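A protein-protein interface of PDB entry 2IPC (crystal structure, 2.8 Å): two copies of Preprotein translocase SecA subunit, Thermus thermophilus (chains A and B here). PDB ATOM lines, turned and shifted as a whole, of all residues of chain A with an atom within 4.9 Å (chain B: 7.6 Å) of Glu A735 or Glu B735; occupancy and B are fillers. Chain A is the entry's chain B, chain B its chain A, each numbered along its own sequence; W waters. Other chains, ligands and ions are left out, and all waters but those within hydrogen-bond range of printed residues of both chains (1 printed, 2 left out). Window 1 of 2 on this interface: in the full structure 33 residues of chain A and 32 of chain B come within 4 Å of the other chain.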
ATOM      1  N   ASP A 419       9.610  20.521 -14.188  1.00  0.00           N
ATOM      2  CA  ASP A 419       9.648  21.159 -12.899  1.00  0.00           C
ATOM      3  C   ASP A 419      11.059  21.488 -12.673  1.00  0.00           C
ATOM      4  O   ASP A 419      11.906  21.147 -13.500  1.00  0.00           O
ATOM      5  CB  ASP A 419       9.125  20.239 -11.812  1.00  0.00           C
ATOM      6  CG  ASP A 419       7.629  20.180 -11.825  1.00  0.00           C
ATOM      7  OD1 ASP A 419       7.010  21.152 -12.370  1.00  0.00           O
ATOM      8  OD2 ASP A 419       7.077  19.181 -11.312  1.00  0.00           O
ATOM      9  N   ARG A 668       3.876  22.603  -5.902  1.00  0.00           N
ATOM     10  CA  ARG A 668       2.744  21.879  -6.460  1.00  0.00           C
ATOM     11  C   ARG A 668       1.615  21.661  -5.477  1.00  0.00           C
ATOM     12  O   ARG A 668       1.847  21.513  -4.281  1.00  0.00           O
ATOM     13  CB  ARG A 668       3.227  20.575  -7.078  1.00  0.00           C
ATOM     14  CG  ARG A 668       4.213  20.823  -8.202  1.00  0.00           C
ATOM     15  CD  ARG A 668       4.766  19.528  -8.709  1.00  0.00           C
ATOM     16  NE  ARG A 668       3.734  18.647  -9.229  1.00  0.00           N
ATOM     17  CZ  ARG A 668       3.992  17.544  -9.918  1.00  0.00           C
ATOM     18  NH1 ARG A 668       5.234  17.195 -10.168  1.00  0.00           N
ATOM     19  NH2 ARG A 668       3.006  16.793 -10.358  1.00  0.00           N
ATOM     20  N   PRO A 728      16.535  10.489 -10.550  1.00  0.00           N
ATOM     21  CA  PRO A 728      15.372   9.594 -10.588  1.00  0.00           C
ATOM     22  C   PRO A 728      14.591   9.493  -9.270  1.00  0.00           C
ATOM     23  O   PRO A 728      13.379   9.698  -9.223  1.00  0.00           O
ATOM     24  CB  PRO A 728      15.989   8.259 -10.962  1.00  0.00           C
ATOM     25  CG  PRO A 728      17.195   8.635 -11.744  1.00  0.00           C
ATOM     26  CD  PRO A 728      17.754   9.817 -11.044  1.00  0.00           C
ATOM     27  N   THR A 731      12.526  12.786  -8.719  1.00  0.00           N
ATOM     28  CA  THR A 731      11.315  12.971  -9.499  1.00  0.00           C
ATOM     29  C   THR A 731      10.326  11.830  -9.255  1.00  0.00           C
ATOM     30  O   THR A 731       9.120  12.003  -9.431  1.00  0.00           O
ATOM     31  CB  THR A 731      11.588  13.084 -10.996  1.00  0.00           C
ATOM     32  OG1 THR A 731      11.026  11.944 -11.655  1.00  0.00           O
ATOM     33  CG2 THR A 731      13.063  13.195 -11.272  1.00  0.00           C
ATOM     34  N   ARG A 732      10.838  10.665  -8.868  1.00  0.00           N
ATOM     35  CA  ARG A 732       9.986   9.511  -8.548  1.00  0.00           C
ATOM     36  C   ARG A 732       9.165   9.891  -7.313  1.00  0.00           C
ATOM     37  O   ARG A 732       7.942   9.867  -7.323  1.00  0.00           O
ATOM     38  CB  ARG A 732      10.829   8.290  -8.161  1.00  0.00           C
ATOM     39  CG  ARG A 732      10.727   7.048  -9.023  1.00  0.00           C
ATOM     40  CD  ARG A 732      11.255   5.871  -8.242  1.00  0.00           C
ATOM     41  NE  ARG A 732      12.468   5.329  -8.853  1.00  0.00           N
ATOM     42  CZ  ARG A 732      12.512   4.529  -9.935  1.00  0.00           C
ATOM     43  NH1 ARG A 732      11.388   4.179 -10.541  1.00  0.00           N
ATOM     44  NH2 ARG A 732      13.672   3.996 -10.393  1.00  0.00           N
ATOM     45  N   SER A 733       9.857  10.253  -6.238  1.00  0.00           N
ATOM     46  CA  SER A 733       9.173  10.596  -5.013  1.00  0.00           C
ATOM     47  C   SER A 733       8.251  11.789  -5.115  1.00  0.00           C
ATOM     48  O   SER A 733       7.205  11.806  -4.482  1.00  0.00           O
ATOM     49  CB  SER A 733      10.170  10.752  -3.871  1.00  0.00           C
ATOM     50  OG  SER A 733      11.336  11.371  -4.304  1.00  0.00           O
ATOM     51  N   ILE A 734       8.592  12.779  -5.915  1.00  0.00           N
ATOM     52  CA  ILE A 734       7.674  13.905  -6.041  1.00  0.00           C
ATOM     53  C   ILE A 734       6.373  13.453  -6.702  1.00  0.00           C
ATOM     54  O   ILE A 734       5.312  13.494  -6.095  1.00  0.00           O
ATOM     55  CB  ILE A 734       8.258  15.014  -6.879  1.00  0.00           C
ATOM     56  CG1 ILE A 734       9.517  15.533  -6.212  1.00  0.00           C
ATOM     57  CG2 ILE A 734       7.260  16.152  -6.990  1.00  0.00           C
ATOM     58  CD1 ILE A 734      10.191  16.611  -7.016  1.00  0.00           C
ATOM     59  N   GLU A 735       6.458  13.018  -7.944  1.00  0.00           N
ATOM     60  CA  GLU A 735       5.272  12.588  -8.638  1.00  0.00           C
ATOM     61  C   GLU A 735       4.450  11.594  -7.836  1.00  0.00           C
ATOM     62  O   GLU A 735       3.226  11.561  -7.955  1.00  0.00           O
ATOM     63  CB  GLU A 735       5.678  12.043  -9.980  1.00  0.00           C
ATOM     64  CG  GLU A 735       6.398  13.160 -10.757  1.00  0.00           C
ATOM     65  CD  GLU A 735       5.470  14.334 -11.129  1.00  0.00           C
ATOM     66  OE1 GLU A 735       5.970  15.325 -11.729  1.00  0.00           O
ATOM     67  OE2 GLU A 735       4.257  14.263 -10.838  1.00  0.00           O
ATOM     68  N   ARG A 736       5.107  10.816  -6.982  1.00  0.00           N
ATOM     69  CA  ARG A 736       4.381   9.858  -6.168  1.00  0.00           C
ATOM     70  C   ARG A 736       3.754  10.490  -4.933  1.00  0.00           C
ATOM     71  O   ARG A 736       2.691  10.075  -4.491  1.00  0.00           O
ATOM     72  CB  ARG A 736       5.287   8.680  -5.777  1.00  0.00           C
ATOM     73  CG  ARG A 736       5.580   7.685  -6.940  1.00  0.00           C
ATOM     74  CD  ARG A 736       5.967   6.283  -6.454  1.00  0.00           C
ATOM     75  NE  ARG A 736       6.525   5.430  -7.504  1.00  0.00           N
ATOM     76  CZ  ARG A 736       6.753   4.121  -7.375  1.00  0.00           C
ATOM     77  NH1 ARG A 736       6.467   3.501  -6.244  1.00  0.00           N
ATOM     78  NH2 ARG A 736       7.288   3.427  -8.370  1.00  0.00           N
ATOM     79  N   ALA A 737       4.388  11.500  -4.364  1.00  0.00           N
ATOM     80  CA  ALA A 737       3.799  12.131  -3.199  1.00  0.00           C
ATOM     81  C   ALA A 737       2.475  12.766  -3.561  1.00  0.00           C
ATOM     82  O   ALA A 737       1.512  12.559  -2.868  1.00  0.00           O
ATOM     83  CB  ALA A 737       4.728  13.168  -2.655  1.00  0.00           C
ATOM     84  N   GLN A 738       2.431  13.538  -4.643  1.00  0.00           N
ATOM     85  CA  GLN A 738       1.198  14.184  -5.057  1.00  0.00           C
ATOM     86  C   GLN A 738       0.123  13.152  -5.237  1.00  0.00           C
ATOM     87  O   GLN A 738      -1.045  13.453  -5.031  1.00  0.00           O
ATOM     88  CB  GLN A 738       1.361  14.940  -6.369  1.00  0.00           C
ATOM     89  CG  GLN A 738       0.120  15.730  -6.716  1.00  0.00           C
ATOM     90  CD  GLN A 738       0.358  16.854  -7.692  1.00  0.00           C
ATOM     91  OE1 GLN A 738       0.606  16.633  -8.849  1.00  0.00           O
ATOM     92  NE2 GLN A 738       0.267  18.066  -7.220  1.00  0.00           N
ATOM     93  N   LYS A 739       0.503  11.935  -5.614  1.00  0.00           N
ATOM     94  CA  LYS A 739      -0.506  10.904  -5.796  1.00  0.00           C
ATOM     95  C   LYS A 739      -0.953  10.336  -4.465  1.00  0.00           C
ATOM     96  O   LYS A 739      -2.091   9.909  -4.344  1.00  0.00           O
ATOM     97  CB  LYS A 739      -0.025   9.764  -6.690  1.00  0.00           C
ATOM     98  CG  LYS A 739      -1.157   8.825  -7.100  1.00  0.00           C
ATOM     99  CD  LYS A 739      -0.604   7.553  -7.700  1.00  0.00           C
ATOM    100  CE  LYS A 739      -1.357   7.173  -8.991  1.00  0.00           C
ATOM    101  NZ  LYS A 739      -0.869   5.918  -9.744  1.00  0.00           N
ATOM    102  N   ASP B 419      15.673  10.319 -16.547  1.00  0.00           N
ATOM    103  CA  ASP B 419      15.243   9.469 -17.633  1.00  0.00           C
ATOM    104  C   ASP B 419      15.302  10.311 -18.875  1.00  0.00           C
ATOM    105  O   ASP B 419      15.553  11.512 -18.802  1.00  0.00           O
ATOM    106  CB  ASP B 419      13.821   8.954 -17.402  1.00  0.00           C
ATOM    107  CG  ASP B 419      13.732   7.962 -16.243  1.00  0.00           C
ATOM    108  OD1 ASP B 419      14.653   7.914 -15.388  1.00  0.00           O
ATOM    109  OD2 ASP B 419      12.719   7.234 -16.181  1.00  0.00           O
ATOM    110  N   ARG B 668      11.719   1.046 -18.406  1.00  0.00           N
ATOM    111  CA  ARG B 668      11.565   0.794 -16.980  1.00  0.00           C
ATOM    112  C   ARG B 668      10.745  -0.429 -16.707  1.00  0.00           C
ATOM    113  O   ARG B 668       9.792  -0.748 -17.424  1.00  0.00           O
ATOM    114  CB  ARG B 668      10.965   1.998 -16.270  1.00  0.00           C
ATOM    115  CG  ARG B 668      11.923   3.130 -16.251  1.00  0.00           C
ATOM    116  CD  ARG B 668      11.292   4.380 -15.769  1.00  0.00           C
ATOM    117  NE  ARG B 668      11.120   4.389 -14.341  1.00  0.00           N
ATOM    118  CZ  ARG B 668      10.793   5.481 -13.675  1.00  0.00           C
ATOM    119  NH1 ARG B 668      10.620   6.627 -14.318  1.00  0.00           N
ATOM    120  NH2 ARG B 668      10.592   5.420 -12.380  1.00  0.00           N
ATOM    121  N   ARG B 672      10.107  -0.048  -9.275  1.00  0.00           N
ATOM    122  CA  ARG B 672      11.279   0.747  -9.047  1.00  0.00           C
ATOM    123  C   ARG B 672      12.412  -0.122  -8.544  1.00  0.00           C
ATOM    124  O   ARG B 672      13.552   0.088  -8.905  1.00  0.00           O
ATOM    125  CB  ARG B 672      10.978   1.886  -8.059  1.00  0.00           C
ATOM    126  CG  ARG B 672      10.171   1.536  -6.810  1.00  0.00           C
ATOM    127  CD  ARG B 672      10.070   2.726  -5.839  1.00  0.00           C
ATOM    128  NE  ARG B 672       9.066   2.527  -4.775  1.00  0.00           N
ATOM    129  CZ  ARG B 672       8.882   3.327  -3.706  1.00  0.00           C
ATOM    130  NH1 ARG B 672       9.624   4.410  -3.503  1.00  0.00           N
ATOM    131  NH2 ARG B 672       7.947   3.058  -2.797  1.00  0.00           N
ATOM    132  N   ASP B 675      14.330  -2.088 -11.140  1.00  0.00           N
ATOM    133  CA  ASP B 675      15.125  -1.354 -12.077  1.00  0.00           C
ATOM    134  C   ASP B 675      16.219  -0.600 -11.324  1.00  0.00           C
ATOM    135  O   ASP B 675      17.186  -0.117 -11.923  1.00  0.00           O
ATOM    136  CB  ASP B 675      14.201  -0.469 -12.972  1.00  0.00           C
ATOM    137  CG  ASP B 675      13.941   0.957 -12.389  1.00  0.00           C
ATOM    138  OD1 ASP B 675      12.861   1.571 -12.622  1.00  0.00           O
ATOM    139  OD2 ASP B 675      14.837   1.507 -11.712  1.00  0.00           O
ATOM    140  N   ARG B 679      20.662  -0.376 -12.166  1.00  0.00           N
ATOM    141  CA  ARG B 679      21.554   0.735 -11.884  1.00  0.00           C
ATOM    142  C   ARG B 679      22.536   0.246 -10.843  1.00  0.00           C
ATOM    143  O   ARG B 679      23.706   0.653 -10.816  1.00  0.00           O
ATOM    144  CB  ARG B 679      20.768   1.899 -11.329  1.00  0.00           C
ATOM    145  CG  ARG B 679      19.867   2.487 -12.347  1.00  0.00           C
ATOM    146  CD  ARG B 679      19.508   3.869 -11.925  1.00  0.00           C
ATOM    147  NE  ARG B 679      18.162   3.838 -11.436  1.00  0.00           N
ATOM    148  CZ  ARG B 679      17.186   4.552 -11.961  1.00  0.00           C
ATOM    149  NH1 ARG B 679      17.414   5.352 -12.983  1.00  0.00           N
ATOM    150  NH2 ARG B 679      15.969   4.456 -11.473  1.00  0.00           N
ATOM    151  N   LEU B 701       5.578  -0.591 -20.133  1.00  0.00           N
ATOM    152  CA  LEU B 701       5.016   0.136 -19.010  1.00  0.00           C
ATOM    153  C   LEU B 701       3.883   1.038 -19.384  1.00  0.00           C
ATOM    154  O   LEU B 701       2.768   0.920 -18.884  1.00  0.00           O
ATOM    155  CB  LEU B 701       6.121   0.933 -18.319  1.00  0.00           C
ATOM    156  CG  LEU B 701       6.056   1.333 -16.833  1.00  0.00           C
ATOM    157  CD1 LEU B 701       5.813   2.820 -16.733  1.00  0.00           C
ATOM    158  CD2 LEU B 701       5.013   0.573 -16.067  1.00  0.00           C
ATOM    159  N   MET B 702       4.170   1.892 -20.339  1.00  0.00           N
ATOM    160  CA  MET B 702       3.212   2.855 -20.799  1.00  0.00           C
ATOM    161  C   MET B 702       1.975   2.405 -21.514  1.00  0.00           C
ATOM    162  O   MET B 702       1.029   3.163 -21.618  1.00  0.00           O
ATOM    163  CB  MET B 702       3.922   3.890 -21.647  1.00  0.00           C
ATOM    164  CG  MET B 702       4.880   4.671 -20.823  1.00  0.00           C
ATOM    165  SD  MET B 702       4.028   5.283 -19.372  1.00  0.00           S
ATOM    166  CE  MET B 702       3.502   6.929 -19.983  1.00  0.00           C
ATOM    167  N   HIS B 727       8.199  17.218 -20.256  1.00  0.00           N
ATOM    168  CA  HIS B 727       6.896  17.796 -19.984  1.00  0.00           C
ATOM    169  C   HIS B 727       6.325  17.224 -18.691  1.00  0.00           C
ATOM    170  O   HIS B 727       6.420  16.035 -18.430  1.00  0.00           O
ATOM    171  CB  HIS B 727       5.996  17.461 -21.158  1.00  0.00           C
ATOM    172  CG  HIS B 727       4.736  18.246 -21.217  1.00  0.00           C
ATOM    173  ND1 HIS B 727       4.575  19.328 -22.052  1.00  0.00           N
ATOM    174  CD2 HIS B 727       3.533  18.042 -20.630  1.00  0.00           C
ATOM    175  CE1 HIS B 727       3.326  19.750 -21.992  1.00  0.00           C
ATOM    176  NE2 HIS B 727       2.675  18.981 -21.135  1.00  0.00           N
ATOM    177  N   PRO B 728       5.696  18.064 -17.872  1.00  0.00           N
ATOM    178  CA  PRO B 728       5.121  17.623 -16.603  1.00  0.00           C
ATOM    179  C   PRO B 728       4.142  16.501 -16.745  1.00  0.00           C
ATOM    180  O   PRO B 728       4.228  15.521 -16.043  1.00  0.00           O
ATOM    181  CB  PRO B 728       4.439  18.864 -16.085  1.00  0.00           C
ATOM    182  CG  PRO B 728       5.199  19.966 -16.762  1.00  0.00           C
ATOM    183  CD  PRO B 728       5.359  19.471 -18.132  1.00  0.00           C
ATOM    184  N   MET B 729       3.203  16.664 -17.659  1.00  0.00           N
ATOM    185  CA  MET B 729       2.187  15.647 -17.892  1.00  0.00           C
ATOM    186  C   MET B 729       2.828  14.323 -18.245  1.00  0.00           C
ATOM    187  O   MET B 729       2.302  13.250 -17.927  1.00  0.00           O
ATOM    188  CB  MET B 729       1.277  16.070 -19.034  1.00  0.00           C
ATOM    189  CG  MET B 729      -0.106  15.435 -19.007  1.00  0.00           C
ATOM    190  SD  MET B 729      -0.346  14.028 -20.168  1.00  0.00           S
ATOM    191  CE  MET B 729       0.784  14.474 -21.507  1.00  0.00           C
ATOM    192  N   VAL B 730       3.973  14.404 -18.910  1.00  0.00           N
ATOM    193  CA  VAL B 730       4.686  13.205 -19.302  1.00  0.00           C
ATOM    194  C   VAL B 730       5.368  12.550 -18.118  1.00  0.00           C
ATOM    195  O   VAL B 730       5.064  11.401 -17.786  1.00  0.00           O
ATOM    196  CB  VAL B 730       5.736  13.524 -20.351  1.00  0.00           C
ATOM    197  CG1 VAL B 730       6.596  12.297 -20.627  1.00  0.00           C
ATOM    198  CG2 VAL B 730       5.050  13.977 -21.629  1.00  0.00           C
ATOM    199  N   THR B 731       6.275  13.276 -17.475  1.00  0.00           N
ATOM    200  CA  THR B 731       6.976  12.695 -16.354  1.00  0.00           C
ATOM    201  C   THR B 731       5.978  12.287 -15.272  1.00  0.00           C
ATOM    202  O   THR B 731       6.226  11.345 -14.525  1.00  0.00           O
ATOM    203  CB  THR B 731       8.010  13.654 -15.815  1.00  0.00           C
ATOM    204  OG1 THR B 731       7.414  14.464 -14.809  1.00  0.00           O
ATOM    205  CG2 THR B 731       8.480  14.590 -16.924  1.00  0.00           C
ATOM    206  N   ARG B 732       4.837  12.980 -15.200  1.00  0.00           N
ATOM    207  CA  ARG B 732       3.782  12.645 -14.213  1.00  0.00           C
ATOM    208  C   ARG B 732       3.254  11.267 -14.530  1.00  0.00           C
ATOM    209  O   ARG B 732       3.256  10.361 -13.690  1.00  0.00           O
ATOM    210  CB  ARG B 732       2.569  13.610 -14.273  1.00  0.00           C
ATOM    211  CG  ARG B 732       2.667  14.812 -13.376  1.00  0.00           C
ATOM    212  CD  ARG B 732       1.438  15.748 -13.316  1.00  0.00           C
ATOM    213  NE  ARG B 732       1.912  16.958 -12.646  1.00  0.00           N
ATOM    214  CZ  ARG B 732       1.245  18.096 -12.502  1.00  0.00           C
ATOM    215  NH1 ARG B 732       0.023  18.211 -12.993  1.00  0.00           N
ATOM    216  NH2 ARG B 732       1.819  19.120 -11.867  1.00  0.00           N
ATOM    217  N   SER B 733       2.801  11.124 -15.771  1.00  0.00           N
ATOM    218  CA  SER B 733       2.230   9.863 -16.222  1.00  0.00           C
ATOM    219  C   SER B 733       3.180   8.677 -16.122  1.00  0.00           C
ATOM    220  O   SER B 733       2.761   7.569 -15.793  1.00  0.00           O
ATOM    221  CB  SER B 733       1.678  10.000 -17.641  1.00  0.00           C
ATOM    222  OG  SER B 733       2.651  10.485 -18.530  1.00  0.00           O
ATOM    223  N   ILE B 734       4.459   8.901 -16.380  1.00  0.00           N
ATOM    224  CA  ILE B 734       5.418   7.813 -16.272  1.00  0.00           C
ATOM    225  C   ILE B 734       5.505   7.330 -14.817  1.00  0.00           C
ATOM    226  O   ILE B 734       5.097   6.213 -14.509  1.00  0.00           O
ATOM    227  CB  ILE B 734       6.826   8.264 -16.747  1.00  0.00           C
ATOM    228  CG1 ILE B 734       6.861   8.362 -18.278  1.00  0.00           C
ATOM    229  CG2 ILE B 734       7.912   7.305 -16.220  1.00  0.00           C
ATOM    230  CD1 ILE B 734       8.168   8.933 -18.831  1.00  0.00           C
ATOM    231  N   GLU B 735       6.051   8.170 -13.934  1.00  0.00           N
ATOM    232  CA  GLU B 735       6.201   7.823 -12.514  1.00  0.00           C
ATOM    233  C   GLU B 735       4.950   7.190 -11.961  1.00  0.00           C
ATOM    234  O   GLU B 735       5.026   6.290 -11.124  1.00  0.00           O
ATOM    235  CB  GLU B 735       6.513   9.054 -11.654  1.00  0.00           C
ATOM    236  CG  GLU B 735       7.863   9.685 -11.882  1.00  0.00           C
ATOM    237  CD  GLU B 735       8.960   8.675 -11.756  1.00  0.00           C
ATOM    238  OE1 GLU B 735      10.091   8.965 -12.217  1.00  0.00           O
ATOM    239  OE2 GLU B 735       8.672   7.591 -11.197  1.00  0.00           O
ATOM    240  N   ARG B 736       3.805   7.660 -12.445  1.00  0.00           N
ATOM    241  CA  ARG B 736       2.531   7.160 -11.994  1.00  0.00           C
ATOM    242  C   ARG B 736       2.130   5.827 -12.571  1.00  0.00           C
ATOM    243  O   ARG B 736       1.421   5.069 -11.930  1.00  0.00           O
ATOM    244  CB  ARG B 736       1.442   8.155 -12.300  1.00  0.00           C
ATOM    245  CG  ARG B 736       1.483   9.388 -11.471  1.00  0.00           C
ATOM    246  CD  ARG B 736       0.064   9.927 -11.356  1.00  0.00           C
ATOM    247  NE  ARG B 736       0.010  11.206 -10.672  1.00  0.00           N
ATOM    248  CZ  ARG B 736      -1.115  11.755 -10.245  1.00  0.00           C
ATOM    249  NH1 ARG B 736      -2.274  11.128 -10.427  1.00  0.00           N
ATOM    250  NH2 ARG B 736      -1.072  12.933  -9.641  1.00  0.00           N
ATOM    251  N   ALA B 737       2.556   5.542 -13.790  1.00  0.00           N
ATOM    252  CA  ALA B 737       2.211   4.258 -14.388  1.00  0.00           C
ATOM    253  C   ALA B 737       2.948   3.150 -13.666  1.00  0.00           C
ATOM    254  O   ALA B 737       2.345   2.153 -13.316  1.00  0.00           O
ATOM    255  CB  ALA B 737       2.558   4.252 -15.829  1.00  0.00           C
ATOM    256  N   GLN B 738       4.245   3.338 -13.413  1.00  0.00           N
ATOM    257  CA  GLN B 738       5.043   2.336 -12.712  1.00  0.00           C
ATOM    258  C   GLN B 738       4.422   2.041 -11.386  1.00  0.00           C
ATOM    259  O   GLN B 738       4.506   0.926 -10.898  1.00  0.00           O
ATOM    260  CB  GLN B 738       6.491   2.783 -12.482  1.00  0.00           C
ATOM    261  CG  GLN B 738       7.298   1.707 -11.730  1.00  0.00           C
ATOM    262  CD  GLN B 738       8.822   1.753 -11.983  1.00  0.00           C
ATOM    263  OE1 GLN B 738       9.547   2.578 -11.413  1.00  0.00           O
ATOM    264  NE2 GLN B 738       9.307   0.859 -12.854  1.00  0.00           N
ATOM    265  N   LYS B 739       3.782   3.037 -10.804  1.00  0.00           N
ATOM    266  CA  LYS B 739       3.144   2.822  -9.522  1.00  0.00           C
ATOM    267  C   LYS B 739       1.850   2.032  -9.658  1.00  0.00           C
ATOM    268  O   LYS B 739       1.519   1.238  -8.789  1.00  0.00           O
ATOM    269  CB  LYS B 739       2.886   4.157  -8.835  1.00  0.00           C
ATOM    270  CG  LYS B 739       2.457   4.050  -7.391  1.00  0.00           C
ATOM    271  CD  LYS B 739       2.416   5.426  -6.732  1.00  0.00           C
ATOM    272  CE  LYS B 739       1.909   5.330  -5.271  1.00  0.00           C
ATOM    273  NZ  LYS B 739       1.675   6.666  -4.580  1.00  0.00           N
ATOM    274  N   ARG B 740       1.114   2.242 -10.742  1.00  0.00           N
ATOM    275  CA  ARG B 740      -0.128   1.505 -10.921  1.00  0.00           C
ATOM    276  C   ARG B 740       0.224   0.029 -10.914  1.00  0.00           C
ATOM    277  O   ARG B 740      -0.374  -0.759 -10.198  1.00  0.00           O
ATOM    278  CB  ARG B 740      -0.796   1.853 -12.260  1.00  0.00           C
ATOM    279  CG  ARG B 740      -1.416   3.251 -12.378  1.00  0.00           C
ATOM    280  CD  ARG B 740      -2.857   3.341 -11.838  1.00  0.00           C
ATOM    281  NE  ARG B 740      -3.440   4.688 -11.979  1.00  0.00           N
ATOM    282  CZ  ARG B 740      -3.643   5.300 -13.151  1.00  0.00           C
ATOM    283  NH1 ARG B 740      -3.303   4.676 -14.279  1.00  0.00           N
ATOM    284  NH2 ARG B 740      -4.188   6.528 -13.211  1.00  0.00           N
ATOM    285  N   GLU B 742       2.953  -1.567  -9.835  1.00  0.00           N
ATOM    286  CA  GLU B 742       3.421  -1.982  -8.537  1.00  0.00           C
ATOM    287  C   GLU B 742       2.220  -2.333  -7.685  1.00  0.00           C
ATOM    288  O   GLU B 742       2.098  -3.454  -7.204  1.00  0.00           O
ATOM    289  CB  GLU B 742       4.245  -0.872  -7.900  1.00  0.00           C
ATOM    290  CG  GLU B 742       5.715  -0.898  -8.343  1.00  0.00           C
ATOM    291  CD  GLU B 742       6.562   0.225  -7.734  1.00  0.00           C
ATOM    292  OE1 GLU B 742       6.160   0.807  -6.700  1.00  0.00           O
ATOM    293  OE2 GLU B 742       7.648   0.533  -8.282  1.00  0.00           O
HETATM  294  O   HOH W   1       8.214  17.597 -14.673  1.00  0.00           O
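Water W1 lies within hydrogen-bond range of the side-chain hydroxyl (OG1) of Thr B731 (3.2 Å) and the backbone NH (N) of Asp A419 (3.3 Å).
The guanidinium group (NH2) of Arg B668 lies within hydrogen-bond range of the side-chain amide oxygen (OE1) of Gln B738 (3.2 Å).
N of Arg B672 sits at hydrogen-bond distance from OE1 of Gln B738, 3.4 Å away.
The side-chain carboxylate (OE1) of Glu B742 is in salt-bridge range of the guanidinium group (NE) of Arg B672.
OD2 of Asp A419 is in salt-bridge range of NH1 of Arg A668, 2.9 Å away.
NH1 of Arg A668 is in salt-bridge range of OE1 of Glu A735, at 2.5 Å.
The side-chain amide oxygen (OE1) of Gln A738 sits at hydrogen-bond distance from the guanidinium group (NH2) of Arg A668 (2.8 Å).
Among the printed residues, merely in contact across the chains: Arg A732 with Glu B735 (3.0 Å), Glu A735 with Arg B732 (3.0 Å), Arg A732 with Arg B672 (3.4 Å), Glu A735 with Thr B731 (3.5 Å), Pro A728 with Arg B679 (3.5 Å), Glu A735 with Glu B735 (3.5 Å), Arg A736 with Lys B739 (3.6 Å), Lys A739 with Arg B740 (3.6 Å), Arg A736 with Gln B738 (3.8 Å), Lys A739 with Lys B739 (3.8 Å) and Gln A738 with Arg B732 (3.99 Å).
Of the printed residues of chain B, Thr A731 touches Glu B735.
Ser A733 touches none of the printed residues of chain B.
Of chain B, only Thr B731, Arg B732 and Glu B735 come within 4 Å of Glu A735.
Printed residues of chain A within 4 Å of Arg B672: Arg A732 (3.4 Å) and Arg A736 (3.1 Å).
Printed residues of chain A within 4 Å of Arg B679: Pro A728 (3.5 Å) and Arg A732 (2.6 Å).
Of the printed residues of chain A, Glu B735 touches Thr A731 (3.2 Å), Arg A732 (3.0 Å) and Glu A735 (3.5 Å).
The nearest residue of chain B that does not touch Glu A735 is Arg B736 (4.2 Å).
The nearest printed residue of chain A that does not touch Glu B735 is Arg A736 (4.01 Å).
Printed residues of chain B that touch a printed residue of chain A: Arg B668, Arg B672, Asp B675, Arg B679, Thr B731, Arg B732, Glu B735, Arg B736, Gln B738, Lys B739, Arg B740 and Glu B742.
Printed residues of chain A that touch a printed residue of chain B: Arg A668, Pro A728, Thr A731, Arg A732, Glu A735, Arg A736, Gln A738 and Lys A739.
Hydrophobic or aromatic side chains of chain A that line the printed part of chain B: Pro A728.
Among the printed residues, 20 pairs touch across the chains.
Among the printed residues, Asp or Glu carboxylates within 4 Å of a Lys or Arg side-chain nitrogen of the other chain: Arg A732 with Asp B675 and Arg A736 with Glu B742.
The guanidinium group (NH2) of Arg A732 is in salt-bridge range of the side-chain carboxylate (OD2) of Asp B675 (3.0 Å).
The guanidinium group (NH2) of Arg B679 lies close to the guanidinium group (NH2) of Arg A732 (2.6 Å).
The guanidinium group (NE) of Arg B732 lies close to the guanidinium group (NH2) of Arg A668, at 2.5 Å.
The side-chain hydroxyl (OG1) of Thr A731 lies within hydrogen-bond range of the side-chain carboxylate (OE1) of Glu B735.
O of Arg B736 lies within hydrogen-bond range of NZ of Lys A739, at 3.3 Å.
The side-chain amide oxygen (OE1) of Gln B738 is in hydrogen-bond range of the guanidinium group (NH1) of Arg A732 (2.6 Å).
NH1 of Arg A736 lies within salt-bridge range of OE1 of Glu B742, 2.7 Å away.
The guanidinium group (NH1) of Arg A732 lies close to the guanidinium group (NH2) of Arg B668 (2.4 Å).
The guanidinium group of Arg B672 lies close to the guanidinium group of Arg A736 (3.1 Å).
Arg A668 touches Arg B732, and with the chains exchanged Arg A732 touches Arg B668.
Arg A732 touches Glu B735, and with the chains exchanged Glu A735 touches Arg B732.
Glu A735 touches its own counterpart, Glu B735.
Arg A736 touches Lys B739, and with the chains exchanged Lys A739 touches Arg B736.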
